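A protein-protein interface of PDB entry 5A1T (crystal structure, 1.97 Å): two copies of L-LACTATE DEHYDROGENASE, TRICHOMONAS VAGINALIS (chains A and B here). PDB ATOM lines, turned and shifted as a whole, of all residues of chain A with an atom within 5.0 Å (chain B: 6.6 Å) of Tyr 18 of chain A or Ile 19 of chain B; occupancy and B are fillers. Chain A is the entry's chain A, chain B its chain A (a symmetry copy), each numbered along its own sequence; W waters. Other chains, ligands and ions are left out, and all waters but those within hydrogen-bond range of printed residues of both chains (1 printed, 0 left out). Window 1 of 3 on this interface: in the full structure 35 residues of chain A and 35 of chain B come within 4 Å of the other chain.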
ATOM      1  N   ALA A  12      -8.146  16.436 -21.569  1.00  0.00           N
ATOM      2  CA  ALA A  12      -6.899  15.744 -21.869  1.00  0.00           C
ATOM      3  C   ALA A  12      -6.380  14.929 -20.689  1.00  0.00           C
ATOM      4  O   ALA A  12      -5.692  13.926 -20.881  1.00  0.00           O
ATOM      5  CB  ALA A  12      -5.845  16.746 -22.304  1.00  0.00           C
ATOM      6  N   GLY A  14      -7.963  13.103 -18.664  1.00  0.00           N
ATOM      7  CA  GLY A  14      -8.726  11.890 -18.421  1.00  0.00           C
ATOM      8  C   GLY A  14      -8.092  10.637 -18.997  1.00  0.00           C
ATOM      9  O   GLY A  14      -6.932  10.646 -19.405  1.00  0.00           O
ATOM     10  N   GLN A  15      -8.865   9.555 -19.028  1.00  0.00           N
ATOM     11  CA  GLN A  15      -8.374   8.256 -19.487  1.00  0.00           C
ATOM     12  C   GLN A  15      -8.119   8.235 -20.993  1.00  0.00           C
ATOM     13  O   GLN A  15      -7.078   7.760 -21.447  1.00  0.00           O
ATOM     14  CB  GLN A  15      -9.370   7.152 -19.123  1.00  0.00           C
ATOM     15  CG  GLN A  15      -9.579   6.967 -17.628  1.00  0.00           C
ATOM     16  CD  GLN A  15      -8.344   6.447 -16.920  1.00  0.00           C
ATOM     17  OE1 GLN A  15      -7.918   7.000 -15.905  1.00  0.00           O
ATOM     18  NE2 GLN A  15      -7.767   5.371 -17.445  1.00  0.00           N
ATOM     19  N   ILE A  16      -9.079   8.739 -21.763  1.00  0.00           N
ATOM     20  CA  ILE A  16      -8.944   8.793 -23.214  1.00  0.00           C
ATOM     21  C   ILE A  16      -7.896   9.828 -23.619  1.00  0.00           C
ATOM     22  O   ILE A  16      -7.055   9.562 -24.475  1.00  0.00           O
ATOM     23  CB  ILE A  16     -10.296   9.113 -23.891  1.00  0.00           C
ATOM     24  CG1 ILE A  16     -11.249   7.925 -23.737  1.00  0.00           C
ATOM     25  CG2 ILE A  16     -10.104   9.440 -25.380  1.00  0.00           C
ATOM     26  CD1 ILE A  16     -12.665   8.184 -24.227  1.00  0.00           C
ATOM     27  N   GLY A  17      -7.950  11.005 -23.005  1.00  0.00           N
ATOM     28  CA  GLY A  17      -7.019  12.075 -23.322  1.00  0.00           C
ATOM     29  C   GLY A  17      -5.577  11.670 -23.078  1.00  0.00           C
ATOM     30  O   GLY A  17      -4.670  12.107 -23.785  1.00  0.00           O
ATOM     31  N   TYR A  18      -5.377  10.829 -22.069  1.00  0.00           N
ATOM     32  CA  TYR A  18      -4.060  10.303 -21.732  1.00  0.00           C
ATOM     33  C   TYR A  18      -3.449   9.540 -22.904  1.00  0.00           C
ATOM     34  O   TYR A  18      -2.345   9.852 -23.360  1.00  0.00           O
ATOM     35  CB  TYR A  18      -4.165   9.395 -20.501  1.00  0.00           C
ATOM     36  CG  TYR A  18      -2.861   8.787 -20.045  1.00  0.00           C
ATOM     37  CD1 TYR A  18      -1.867   9.569 -19.469  1.00  0.00           C
ATOM     38  CD2 TYR A  18      -2.633   7.427 -20.170  1.00  0.00           C
ATOM     39  CE1 TYR A  18      -0.680   9.012 -19.046  1.00  0.00           C
ATOM     40  CE2 TYR A  18      -1.450   6.860 -19.749  1.00  0.00           C
ATOM     41  CZ  TYR A  18      -0.477   7.655 -19.187  1.00  0.00           C
ATOM     42  OH  TYR A  18       0.703   7.090 -18.766  1.00  0.00           O
ATOM     43  N   ILE A  19      -4.183   8.547 -23.393  1.00  0.00           N
ATOM     44  CA  ILE A  19      -3.704   7.697 -24.476  1.00  0.00           C
ATOM     45  C   ILE A  19      -3.715   8.447 -25.804  1.00  0.00           C
ATOM     46  O   ILE A  19      -2.781   8.331 -26.599  1.00  0.00           O
ATOM     47  CB  ILE A  19      -4.562   6.421 -24.609  1.00  0.00           C
ATOM     48  CG1 ILE A  19      -4.638   5.689 -23.265  1.00  0.00           C
ATOM     49  CG2 ILE A  19      -3.991   5.501 -25.685  1.00  0.00           C
ATOM     50  CD1 ILE A  19      -5.644   4.560 -23.231  1.00  0.00           C
ATOM     51  N   LEU A  20      -4.779   9.212 -26.034  1.00  0.00           N
ATOM     52  CA  LEU A  20      -4.963   9.940 -27.285  1.00  0.00           C
ATOM     53  C   LEU A  20      -3.802  10.885 -27.561  1.00  0.00           C
ATOM     54  O   LEU A  20      -3.288  10.943 -28.678  1.00  0.00           O
ATOM     55  CB  LEU A  20      -6.277  10.725 -27.248  1.00  0.00           C
ATOM     56  CG  LEU A  20      -6.629  11.549 -28.490  1.00  0.00           C
ATOM     57  CD1 LEU A  20      -6.851  10.648 -29.690  1.00  0.00           C
ATOM     58  CD2 LEU A  20      -7.859  12.409 -28.225  1.00  0.00           C
ATOM     59  N   SER A  21      -3.394  11.621 -26.534  1.00  0.00           N
ATOM     60  CA  SER A  21      -2.296  12.573 -26.657  1.00  0.00           C
ATOM     61  C   SER A  21      -0.996  11.881 -27.056  1.00  0.00           C
ATOM     62  O   SER A  21      -0.293  12.337 -27.958  1.00  0.00           O
ATOM     63  CB  SER A  21      -2.099  13.330 -25.343  1.00  0.00           C
ATOM     64  OG  SER A  21      -3.239  14.113 -25.030  1.00  0.00           O
ATOM     65  N   HIS A  22      -0.681  10.779 -26.383  1.00  0.00           N
ATOM     66  CA  HIS A  22       0.550  10.044 -26.655  1.00  0.00           C
ATOM     67  C   HIS A  22       0.571   9.441 -28.053  1.00  0.00           C
ATOM     68  O   HIS A  22       1.588   9.501 -28.747  1.00  0.00           O
ATOM     69  CB  HIS A  22       0.748   8.932 -25.624  1.00  0.00           C
ATOM     70  CG  HIS A  22       1.323   9.405 -24.326  1.00  0.00           C
ATOM     71  ND1 HIS A  22       0.548   9.925 -23.313  1.00  0.00           N
ATOM     72  CD2 HIS A  22       2.601   9.439 -23.878  1.00  0.00           C
ATOM     73  CE1 HIS A  22       1.323  10.256 -22.295  1.00  0.00           C
ATOM     74  NE2 HIS A  22       2.572   9.973 -22.613  1.00  0.00           N
ATOM     75  N   LEU A  52       0.389  14.266 -17.363  1.00  0.00           N
ATOM     76  CA  LEU A  52       0.330  13.921 -18.777  1.00  0.00           C
ATOM     77  C   LEU A  52       1.482  14.557 -19.544  1.00  0.00           C
ATOM     78  O   LEU A  52       2.190  13.875 -20.283  1.00  0.00           O
ATOM     79  CB  LEU A  52      -1.003  14.358 -19.392  1.00  0.00           C
ATOM     80  CG  LEU A  52      -1.063  14.271 -20.920  1.00  0.00           C
ATOM     81  CD1 LEU A  52      -0.717  12.866 -21.388  1.00  0.00           C
ATOM     82  CD2 LEU A  52      -2.427  14.686 -21.436  1.00  0.00           C
ATOM     83  N   GLU A  55       4.882  12.998 -18.976  1.00  0.00           N
ATOM     84  CA  GLU A  55       5.082  11.741 -19.683  1.00  0.00           C
ATOM     85  C   GLU A  55       5.264  11.972 -21.180  1.00  0.00           C
ATOM     86  O   GLU A  55       6.024  11.259 -21.829  1.00  0.00           O
ATOM     87  CB  GLU A  55       3.918  10.787 -19.433  1.00  0.00           C
ATOM     88  CG  GLU A  55       3.950  10.157 -18.053  1.00  0.00           C
ATOM     89  CD  GLU A  55       3.355   8.767 -18.033  1.00  0.00           C
ATOM     90  OE1 GLU A  55       3.856   7.893 -18.774  1.00  0.00           O
ATOM     91  OE2 GLU A  55       2.384   8.548 -17.278  1.00  0.00           O
ATOM     92  N   ALA B  12      -0.417  -8.425 -18.617  1.00  0.00           N
ATOM     93  CA  ALA B  12      -1.087  -7.718 -19.701  1.00  0.00           C
ATOM     94  C   ALA B  12      -2.297  -6.921 -19.225  1.00  0.00           C
ATOM     95  O   ALA B  12      -2.652  -5.909 -19.830  1.00  0.00           O
ATOM     96  CB  ALA B  12      -1.511  -8.703 -20.775  1.00  0.00           C
ATOM     97  N   GLY B  14      -2.636  -5.146 -16.641  1.00  0.00           N
ATOM     98  CA  GLY B  14      -2.281  -3.944 -15.906  1.00  0.00           C
ATOM     99  C   GLY B  14      -2.328  -2.675 -16.738  1.00  0.00           C
ATOM    100  O   GLY B  14      -2.854  -2.667 -17.850  1.00  0.00           O
ATOM    101  N   GLN B  15      -1.770  -1.599 -16.190  1.00  0.00           N
ATOM    102  CA  GLN B  15      -1.799  -0.287 -16.838  1.00  0.00           C
ATOM    103  C   GLN B  15      -0.909  -0.236 -18.078  1.00  0.00           C
ATOM    104  O   GLN B  15      -1.322   0.255 -19.128  1.00  0.00           O
ATOM    105  CB  GLN B  15      -1.366   0.802 -15.854  1.00  0.00           C
ATOM    106  CG  GLN B  15      -2.282   0.957 -14.650  1.00  0.00           C
ATOM    107  CD  GLN B  15      -3.659   1.473 -15.020  1.00  0.00           C
ATOM    108  OE1 GLN B  15      -4.675   0.905 -14.619  1.00  0.00           O
ATOM    109  NE2 GLN B  15      -3.700   2.563 -15.780  1.00  0.00           N
ATOM    110  N   ILE B  16       0.318  -0.734 -17.947  1.00  0.00           N
ATOM    111  CA  ILE B  16       1.254  -0.759 -19.065  1.00  0.00           C
ATOM    112  C   ILE B  16       0.813  -1.778 -20.114  1.00  0.00           C
ATOM    113  O   ILE B  16       0.827  -1.489 -21.308  1.00  0.00           O
ATOM    114  CB  ILE B  16       2.689  -1.077 -18.587  1.00  0.00           C
ATOM    115  CG1 ILE B  16       3.241   0.100 -17.779  1.00  0.00           C
ATOM    116  CG2 ILE B  16       3.614  -1.375 -19.776  1.00  0.00           C
ATOM    117  CD1 ILE B  16       4.587  -0.160 -17.121  1.00  0.00           C
ATOM    118  N   GLY B  17       0.423  -2.967 -19.665  1.00  0.00           N
ATOM    119  CA  GLY B  17       0.002  -4.024 -20.570  1.00  0.00           C
ATOM    120  C   GLY B  17      -1.189  -3.612 -21.415  1.00  0.00           C
ATOM    121  O   GLY B  17      -1.322  -4.029 -22.565  1.00  0.00           O
ATOM    122  N   TYR B  18      -2.054  -2.788 -20.832  1.00  0.00           N
ATOM    123  CA  TYR B  18      -3.224  -2.259 -21.521  1.00  0.00           C
ATOM    124  C   TYR B  18      -2.826  -1.469 -22.765  1.00  0.00           C
ATOM    125  O   TYR B  18      -3.277  -1.764 -23.876  1.00  0.00           O
ATOM    126  CB  TYR B  18      -4.032  -1.374 -20.563  1.00  0.00           C
ATOM    127  CG  TYR B  18      -5.278  -0.765 -21.158  1.00  0.00           C
ATOM    128  CD1 TYR B  18      -6.381  -1.550 -21.473  1.00  0.00           C
ATOM    129  CD2 TYR B  18      -5.360   0.599 -21.383  1.00  0.00           C
ATOM    130  CE1 TYR B  18      -7.521  -0.991 -22.009  1.00  0.00           C
ATOM    131  CE2 TYR B  18      -6.496   1.167 -21.917  1.00  0.00           C
ATOM    132  CZ  TYR B  18      -7.573   0.370 -22.227  1.00  0.00           C
ATOM    133  OH  TYR B  18      -8.707   0.935 -22.759  1.00  0.00           O
ATOM    134  N   ILE B  19      -1.971  -0.473 -22.569  1.00  0.00           N
ATOM    135  CA  ILE B  19      -1.544   0.401 -23.655  1.00  0.00           C
ATOM    136  C   ILE B  19      -0.587  -0.324 -24.596  1.00  0.00           C
ATOM    137  O   ILE B  19      -0.680  -0.186 -25.816  1.00  0.00           O
ATOM    138  CB  ILE B  19      -0.857   1.673 -23.115  1.00  0.00           C
ATOM    139  CG1 ILE B  19      -1.764   2.379 -22.103  1.00  0.00           C
ATOM    140  CG2 ILE B  19      -0.501   2.617 -24.261  1.00  0.00           C
ATOM    141  CD1 ILE B  19      -1.089   3.499 -21.342  1.00  0.00           C
ATOM    142  N   LEU B  20       0.330  -1.093 -24.015  1.00  0.00           N
ATOM    143  CA  LEU B  20       1.354  -1.799 -24.778  1.00  0.00           C
ATOM    144  C   LEU B  20       0.741  -2.729 -25.815  1.00  0.00           C
ATOM    145  O   LEU B  20       1.174  -2.763 -26.967  1.00  0.00           O
ATOM    146  CB  LEU B  20       2.259  -2.595 -23.833  1.00  0.00           C
ATOM    147  CG  LEU B  20       3.395  -3.398 -24.472  1.00  0.00           C
ATOM    148  CD1 LEU B  20       4.397  -2.476 -25.142  1.00  0.00           C
ATOM    149  CD2 LEU B  20       4.079  -4.273 -23.428  1.00  0.00           C
ATOM    150  N   SER B  21      -0.270  -3.482 -25.396  1.00  0.00           N
ATOM    151  CA  SER B  21      -0.948  -4.422 -26.281  1.00  0.00           C
ATOM    152  C   SER B  21      -1.584  -3.713 -27.473  1.00  0.00           C
ATOM    153  O   SER B  21      -1.434  -4.146 -28.615  1.00  0.00           O
ATOM    154  CB  SER B  21      -2.014  -5.202 -25.511  1.00  0.00           C
ATOM    155  OG  SER B  21      -1.429  -6.000 -24.495  1.00  0.00           O
ATOM    156  N   HIS B  22      -2.292  -2.621 -27.202  1.00  0.00           N
ATOM    157  CA  HIS B  22      -2.971  -1.872 -28.254  1.00  0.00           C
ATOM    158  C   HIS B  22      -1.997  -1.243 -29.242  1.00  0.00           C
ATOM    159  O   HIS B  22      -2.220  -1.282 -30.453  1.00  0.00           O
ATOM    160  CB  HIS B  22      -3.852  -0.778 -27.649  1.00  0.00           C
ATOM    161  CG  HIS B  22      -5.175  -1.271 -27.154  1.00  0.00           C
ATOM    162  ND1 HIS B  22      -5.346  -1.816 -25.900  1.00  0.00           N
ATOM    163  CD2 HIS B  22      -6.392  -1.303 -27.747  1.00  0.00           C
ATOM    164  CE1 HIS B  22      -6.612  -2.159 -25.741  1.00  0.00           C
ATOM    165  NE2 HIS B  22      -7.267  -1.861 -26.847  1.00  0.00           N
ATOM    166  N   TRP B  23      -0.922  -0.669 -28.712  1.00  0.00           N
ATOM    167  CA  TRP B  23       0.063   0.033 -29.527  1.00  0.00           C
ATOM    168  C   TRP B  23       0.802  -0.941 -30.442  1.00  0.00           C
ATOM    169  O   TRP B  23       1.087  -0.627 -31.597  1.00  0.00           O
ATOM    170  CB  TRP B  23       1.053   0.783 -28.630  1.00  0.00           C
ATOM    171  CG  TRP B  23       1.696   1.974 -29.281  1.00  0.00           C
ATOM    172  CD1 TRP B  23       1.829   2.211 -30.618  1.00  0.00           C
ATOM    173  CD2 TRP B  23       2.287   3.098 -28.616  1.00  0.00           C
ATOM    174  NE1 TRP B  23       2.469   3.407 -30.827  1.00  0.00           N
ATOM    175  CE2 TRP B  23       2.760   3.973 -29.613  1.00  0.00           C
ATOM    176  CE3 TRP B  23       2.463   3.449 -27.273  1.00  0.00           C
ATOM    177  CZ2 TRP B  23       3.397   5.174 -29.312  1.00  0.00           C
ATOM    178  CZ3 TRP B  23       3.097   4.642 -26.976  1.00  0.00           C
ATOM    179  CH2 TRP B  23       3.556   5.491 -27.992  1.00  0.00           C
ATOM    180  N   ILE B  24       1.100  -2.127 -29.922  1.00  0.00           N
ATOM    181  CA  ILE B  24       1.763  -3.163 -30.707  1.00  0.00           C
ATOM    182  C   ILE B  24       0.807  -3.660 -31.785  1.00  0.00           C
ATOM    183  O   ILE B  24       1.178  -3.774 -32.954  1.00  0.00           O
ATOM    184  CB  ILE B  24       2.232  -4.341 -29.823  1.00  0.00           C
ATOM    185  CG1 ILE B  24       3.416  -3.901 -28.959  1.00  0.00           C
ATOM    186  CG2 ILE B  24       2.637  -5.547 -30.684  1.00  0.00           C
ATOM    187  CD1 ILE B  24       3.850  -4.919 -27.928  1.00  0.00           C
ATOM    188  N   LEU B  52      -9.427  -6.268 -21.683  1.00  0.00           N
ATOM    189  CA  LEU B  52      -8.384  -5.897 -22.629  1.00  0.00           C
ATOM    190  C   LEU B  52      -8.645  -6.509 -23.999  1.00  0.00           C
ATOM    191  O   LEU B  52      -8.623  -5.808 -25.009  1.00  0.00           O
ATOM    192  CB  LEU B  52      -7.006  -6.333 -22.123  1.00  0.00           C
ATOM    193  CG  LEU B  52      -5.878  -6.217 -23.153  1.00  0.00           C
ATOM    194  CD1 LEU B  52      -5.800  -4.802 -23.702  1.00  0.00           C
ATOM    195  CD2 LEU B  52      -4.549  -6.634 -22.555  1.00  0.00           C
ATOM    196  N   ARG B 236       0.486  12.038 -11.113  1.00  0.00           N
ATOM    197  CA  ARG B 236      -0.406  11.075 -11.758  1.00  0.00           C
ATOM    198  C   ARG B 236      -1.248  10.295 -10.754  1.00  0.00           C
ATOM    199  O   ARG B 236      -2.407   9.974 -11.023  1.00  0.00           O
ATOM    200  CB  ARG B 236       0.404  10.097 -12.615  1.00  0.00           C
ATOM    201  CG  ARG B 236      -0.409   8.945 -13.199  1.00  0.00           C
ATOM    202  CD  ARG B 236       0.390   8.172 -14.241  1.00  0.00           C
ATOM    203  NE  ARG B 236      -0.170   6.847 -14.506  1.00  0.00           N
ATOM    204  CZ  ARG B 236      -1.162   6.598 -15.357  1.00  0.00           C
ATOM    205  NH1 ARG B 236      -1.731   7.583 -16.040  1.00  0.00           N
ATOM    206  NH2 ARG B 236      -1.591   5.353 -15.524  1.00  0.00           N
ATOM    207  N   THR B 239       2.556   5.343 -10.991  1.00  0.00           N
ATOM    208  CA  THR B 239       3.807   5.461 -11.735  1.00  0.00           C
ATOM    209  C   THR B 239       3.513   5.554 -13.233  1.00  0.00           C
ATOM    210  O   THR B 239       2.375   5.362 -13.660  1.00  0.00           O
ATOM    211  CB  THR B 239       4.750   4.276 -11.457  1.00  0.00           C
ATOM    212  OG1 THR B 239       4.028   3.044 -11.565  1.00  0.00           O
ATOM    213  CG2 THR B 239       5.348   4.388 -10.063  1.00  0.00           C
ATOM    214  N   SER B 240       4.541   5.855 -14.023  1.00  0.00           N
ATOM    215  CA  SER B 240       4.383   6.049 -15.462  1.00  0.00           C
ATOM    216  C   SER B 240       3.821   4.808 -16.155  1.00  0.00           C
ATOM    217  O   SER B 240       3.882   3.703 -15.613  1.00  0.00           O
ATOM    218  CB  SER B 240       5.724   6.429 -16.092  1.00  0.00           C
ATOM    219  OG  SER B 240       6.665   5.377 -15.964  1.00  0.00           O
ATOM    220  N   ALA B 241       3.280   4.996 -17.358  1.00  0.00           N
ATOM    221  CA  ALA B 241       2.665   3.901 -18.102  1.00  0.00           C
ATOM    222  C   ALA B 241       2.794   4.100 -19.611  1.00  0.00           C
ATOM    223  O   ALA B 241       3.300   3.228 -20.315  1.00  0.00           O
ATOM    224  CB  ALA B 241       1.206   3.761 -17.715  1.00  0.00           C
ATOM    225  N   ALA B 242       2.335   5.243 -20.106  1.00  0.00           N
ATOM    226  CA  ALA B 242       2.409   5.530 -21.536  1.00  0.00           C
ATOM    227  C   ALA B 242       3.855   5.726 -21.988  1.00  0.00           C
ATOM    228  O   ALA B 242       4.242   5.262 -23.062  1.00  0.00           O
ATOM    229  CB  ALA B 242       1.584   6.758 -21.873  1.00  0.00           C
ATOM    230  N   SER B 243       4.651   6.407 -21.170  1.00  0.00           N
ATOM    231  CA  SER B 243       6.028   6.711 -21.537  1.00  0.00           C
ATOM    232  C   SER B 243       6.929   5.470 -21.550  1.00  0.00           C
ATOM    233  O   SER B 243       7.726   5.301 -22.471  1.00  0.00           O
ATOM    234  CB  SER B 243       6.605   7.780 -20.601  1.00  0.00           C
ATOM    235  OG  SER B 243       6.161   7.607 -19.267  1.00  0.00           O
ATOM    236  N   PRO B 244       6.814   4.593 -20.539  1.00  0.00           N
ATOM    237  CA  PRO B 244       7.618   3.368 -20.643  1.00  0.00           C
ATOM    238  C   PRO B 244       7.161   2.432 -21.750  1.00  0.00           C
ATOM    239  O   PRO B 244       7.981   1.700 -22.306  1.00  0.00           O
ATOM    240  CB  PRO B 244       7.430   2.706 -19.281  1.00  0.00           C
ATOM    241  CG  PRO B 244       6.163   3.299 -18.734  1.00  0.00           C
ATOM    242  CD  PRO B 244       6.154   4.699 -19.227  1.00  0.00           C
ATOM    243  N   THR B 245       5.865   2.441 -22.047  1.00  0.00           N
ATOM    244  CA  THR B 245       5.334   1.651 -23.148  1.00  0.00           C
ATOM    245  C   THR B 245       6.041   2.053 -24.437  1.00  0.00           C
ATOM    246  O   THR B 245       6.445   1.203 -25.229  1.00  0.00           O
ATOM    247  CB  THR B 245       3.813   1.844 -23.311  1.00  0.00           C
ATOM    248  OG1 THR B 245       3.147   1.459 -22.102  1.00  0.00           O
ATOM    249  CG2 THR B 245       3.282   1.006 -24.460  1.00  0.00           C
ATOM    250  N   ILE B 249       8.624  -0.311 -26.630  1.00  0.00           N
ATOM    251  CA  ILE B 249       8.412  -0.611 -28.041  1.00  0.00           C
ATOM    252  C   ILE B 249       9.612  -0.120 -28.838  1.00  0.00           C
ATOM    253  O   ILE B 249      10.064  -0.785 -29.771  1.00  0.00           O
ATOM    254  CB  ILE B 249       7.110   0.032 -28.570  1.00  0.00           C
ATOM    255  CG1 ILE B 249       5.898  -0.638 -27.916  1.00  0.00           C
ATOM    256  CG2 ILE B 249       7.010  -0.093 -30.093  1.00  0.00           C
ATOM    257  CD1 ILE B 249       4.577   0.052 -28.189  1.00  0.00           C
HETATM  258  O   HOH W   1      -5.932   3.962 -16.135  1.00  0.00           O
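The backbone NH of Ser 243 of chain B sits at hydrogen-bond distance from the side-chain carboxylate of Glu 55 of chain A, 2.9 Å away.
The side-chain carboxylate (OE1) of Glu 55 of chain A is in hydrogen-bond range of the backbone NH (N) of Ala 242 of chain B (3.3 Å).
OE1 of Glu 55 of chain A is in hydrogen-bond range of N of Ala 241 of chain B, 3.3 Å away.
N of Ala 242 of chain B sits at hydrogen-bond distance from OH of Tyr 18 of chain A.
OH of Tyr 18 of chain A lies within hydrogen-bond range of OE2 of Glu 55 of chain A, at 2.7 Å.
The backbone NH of Tyr 18 of chain A is in hydrogen-bond range of the backbone carbonyl oxygen of Ala 12 of chain A (3.3 Å).
The backbone carbonyl oxygen (O) of Tyr 18 of chain B lies within hydrogen-bond range of a ring nitrogen (ND1) of His 22 of chain B (2.9 Å).
N of Tyr 18 of chain B lies within hydrogen-bond range of O of Ala 12 of chain B, 3.3 Å away.
The backbone carbonyl oxygen (O) of Thr 239 of chain B lies within hydrogen-bond range of the guanidinium group (NE) of Arg 236 of chain B.
O of Tyr 18 of chain A is in hydrogen-bond range of ND1 of His 22 of chain A (2.9 Å).
Tyr 18 of chain A touches Ile 19 of chain B (CE2 to CD1, 3.7 Å).
CZ of Tyr 18 of chain A touches NH1 of Arg 236 of chain B, at 3.4 Å.
OH of Tyr 18 of chain A touches CB of Ala 241 of chain B, at 3.5 Å.
Tyr 18 of chain B touches Ile 19 of chain A (CE2 to CD1, 3.7 Å).
His 22 of chain A touches Ala 242 of chain B (NE2 to CB, 3.4 Å).
CD of Arg 236 of chain B touches OE2 of Glu 55 of chain A, at 3.7 Å.
Ser 240 of chain B touches Glu 55 of chain A.
Pro 244 of chain B touches Glu 55 of chain A (CD to OE1, 3.96 Å).
Gly 14 of chain A touches none of the printed residues of chain B.
Printed residues of chain B within 4 Å of Tyr 18 of chain A: Ile 19 (3.7 Å), Arg 236 (3.4 Å), Ala 241 (3.5 Å) and Ala 242 (2.8 Å).
Of the printed residues of chain B, Ile 19 of chain A touches Tyr 18.
Of the printed residues of chain B, Glu 55 of chain A touches Arg 236 (3.7 Å), Ser 240 (3.6 Å), Ala 241 (3.3 Å), Ala 242 (3.3 Å), Ser 243 (2.4 Å) and Pro 244 (3.96 Å).
Gly 14 of chain B touches none of the printed residues of chain A.
Of the printed residues of chain A, Ile 19 of chain B touches Tyr 18 (3.7 Å).
Printed residues of chain A within 4 Å of Arg 236 of chain B: Tyr 18 and Glu 55.
Printed residues of chain A within 4 Å of Pro 244 of chain B: Glu 55 (3.96 Å).
The nearest printed residue of chain A that does not touch Ile 19 of chain B is Ile 19 of chain A (4.5 Å).
Of the 12 printed residues of chain A, 4 touch a printed residue of chain B.
Printed residues of chain B that touch a printed residue of chain A: Tyr 18, Ile 19, Arg 236, Ser 240, Ala 241, Ala 242, Ser 243 and Pro 244.
Along chain B the printed residues that touch a printed residue of chain A span positions 18 to 244.
Among the printed residues, 12 pairs touch across the chains.
Among the printed residues, no Asp or Glu carboxylate lies within 4 Å of a Lys or Arg side-chain nitrogen of the other chain.
Tyr 18 of chain A touches Ile 19 of chain B, and with the chains exchanged Ile 19 of chain A touches Tyr 18 of chain B.
Water W1 bridges the side-chain amide nitrogen of Gln 15 of chain A (2.7 Å) and the side-chain amide nitrogen of Gln 15 of chain B (2.7 Å).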
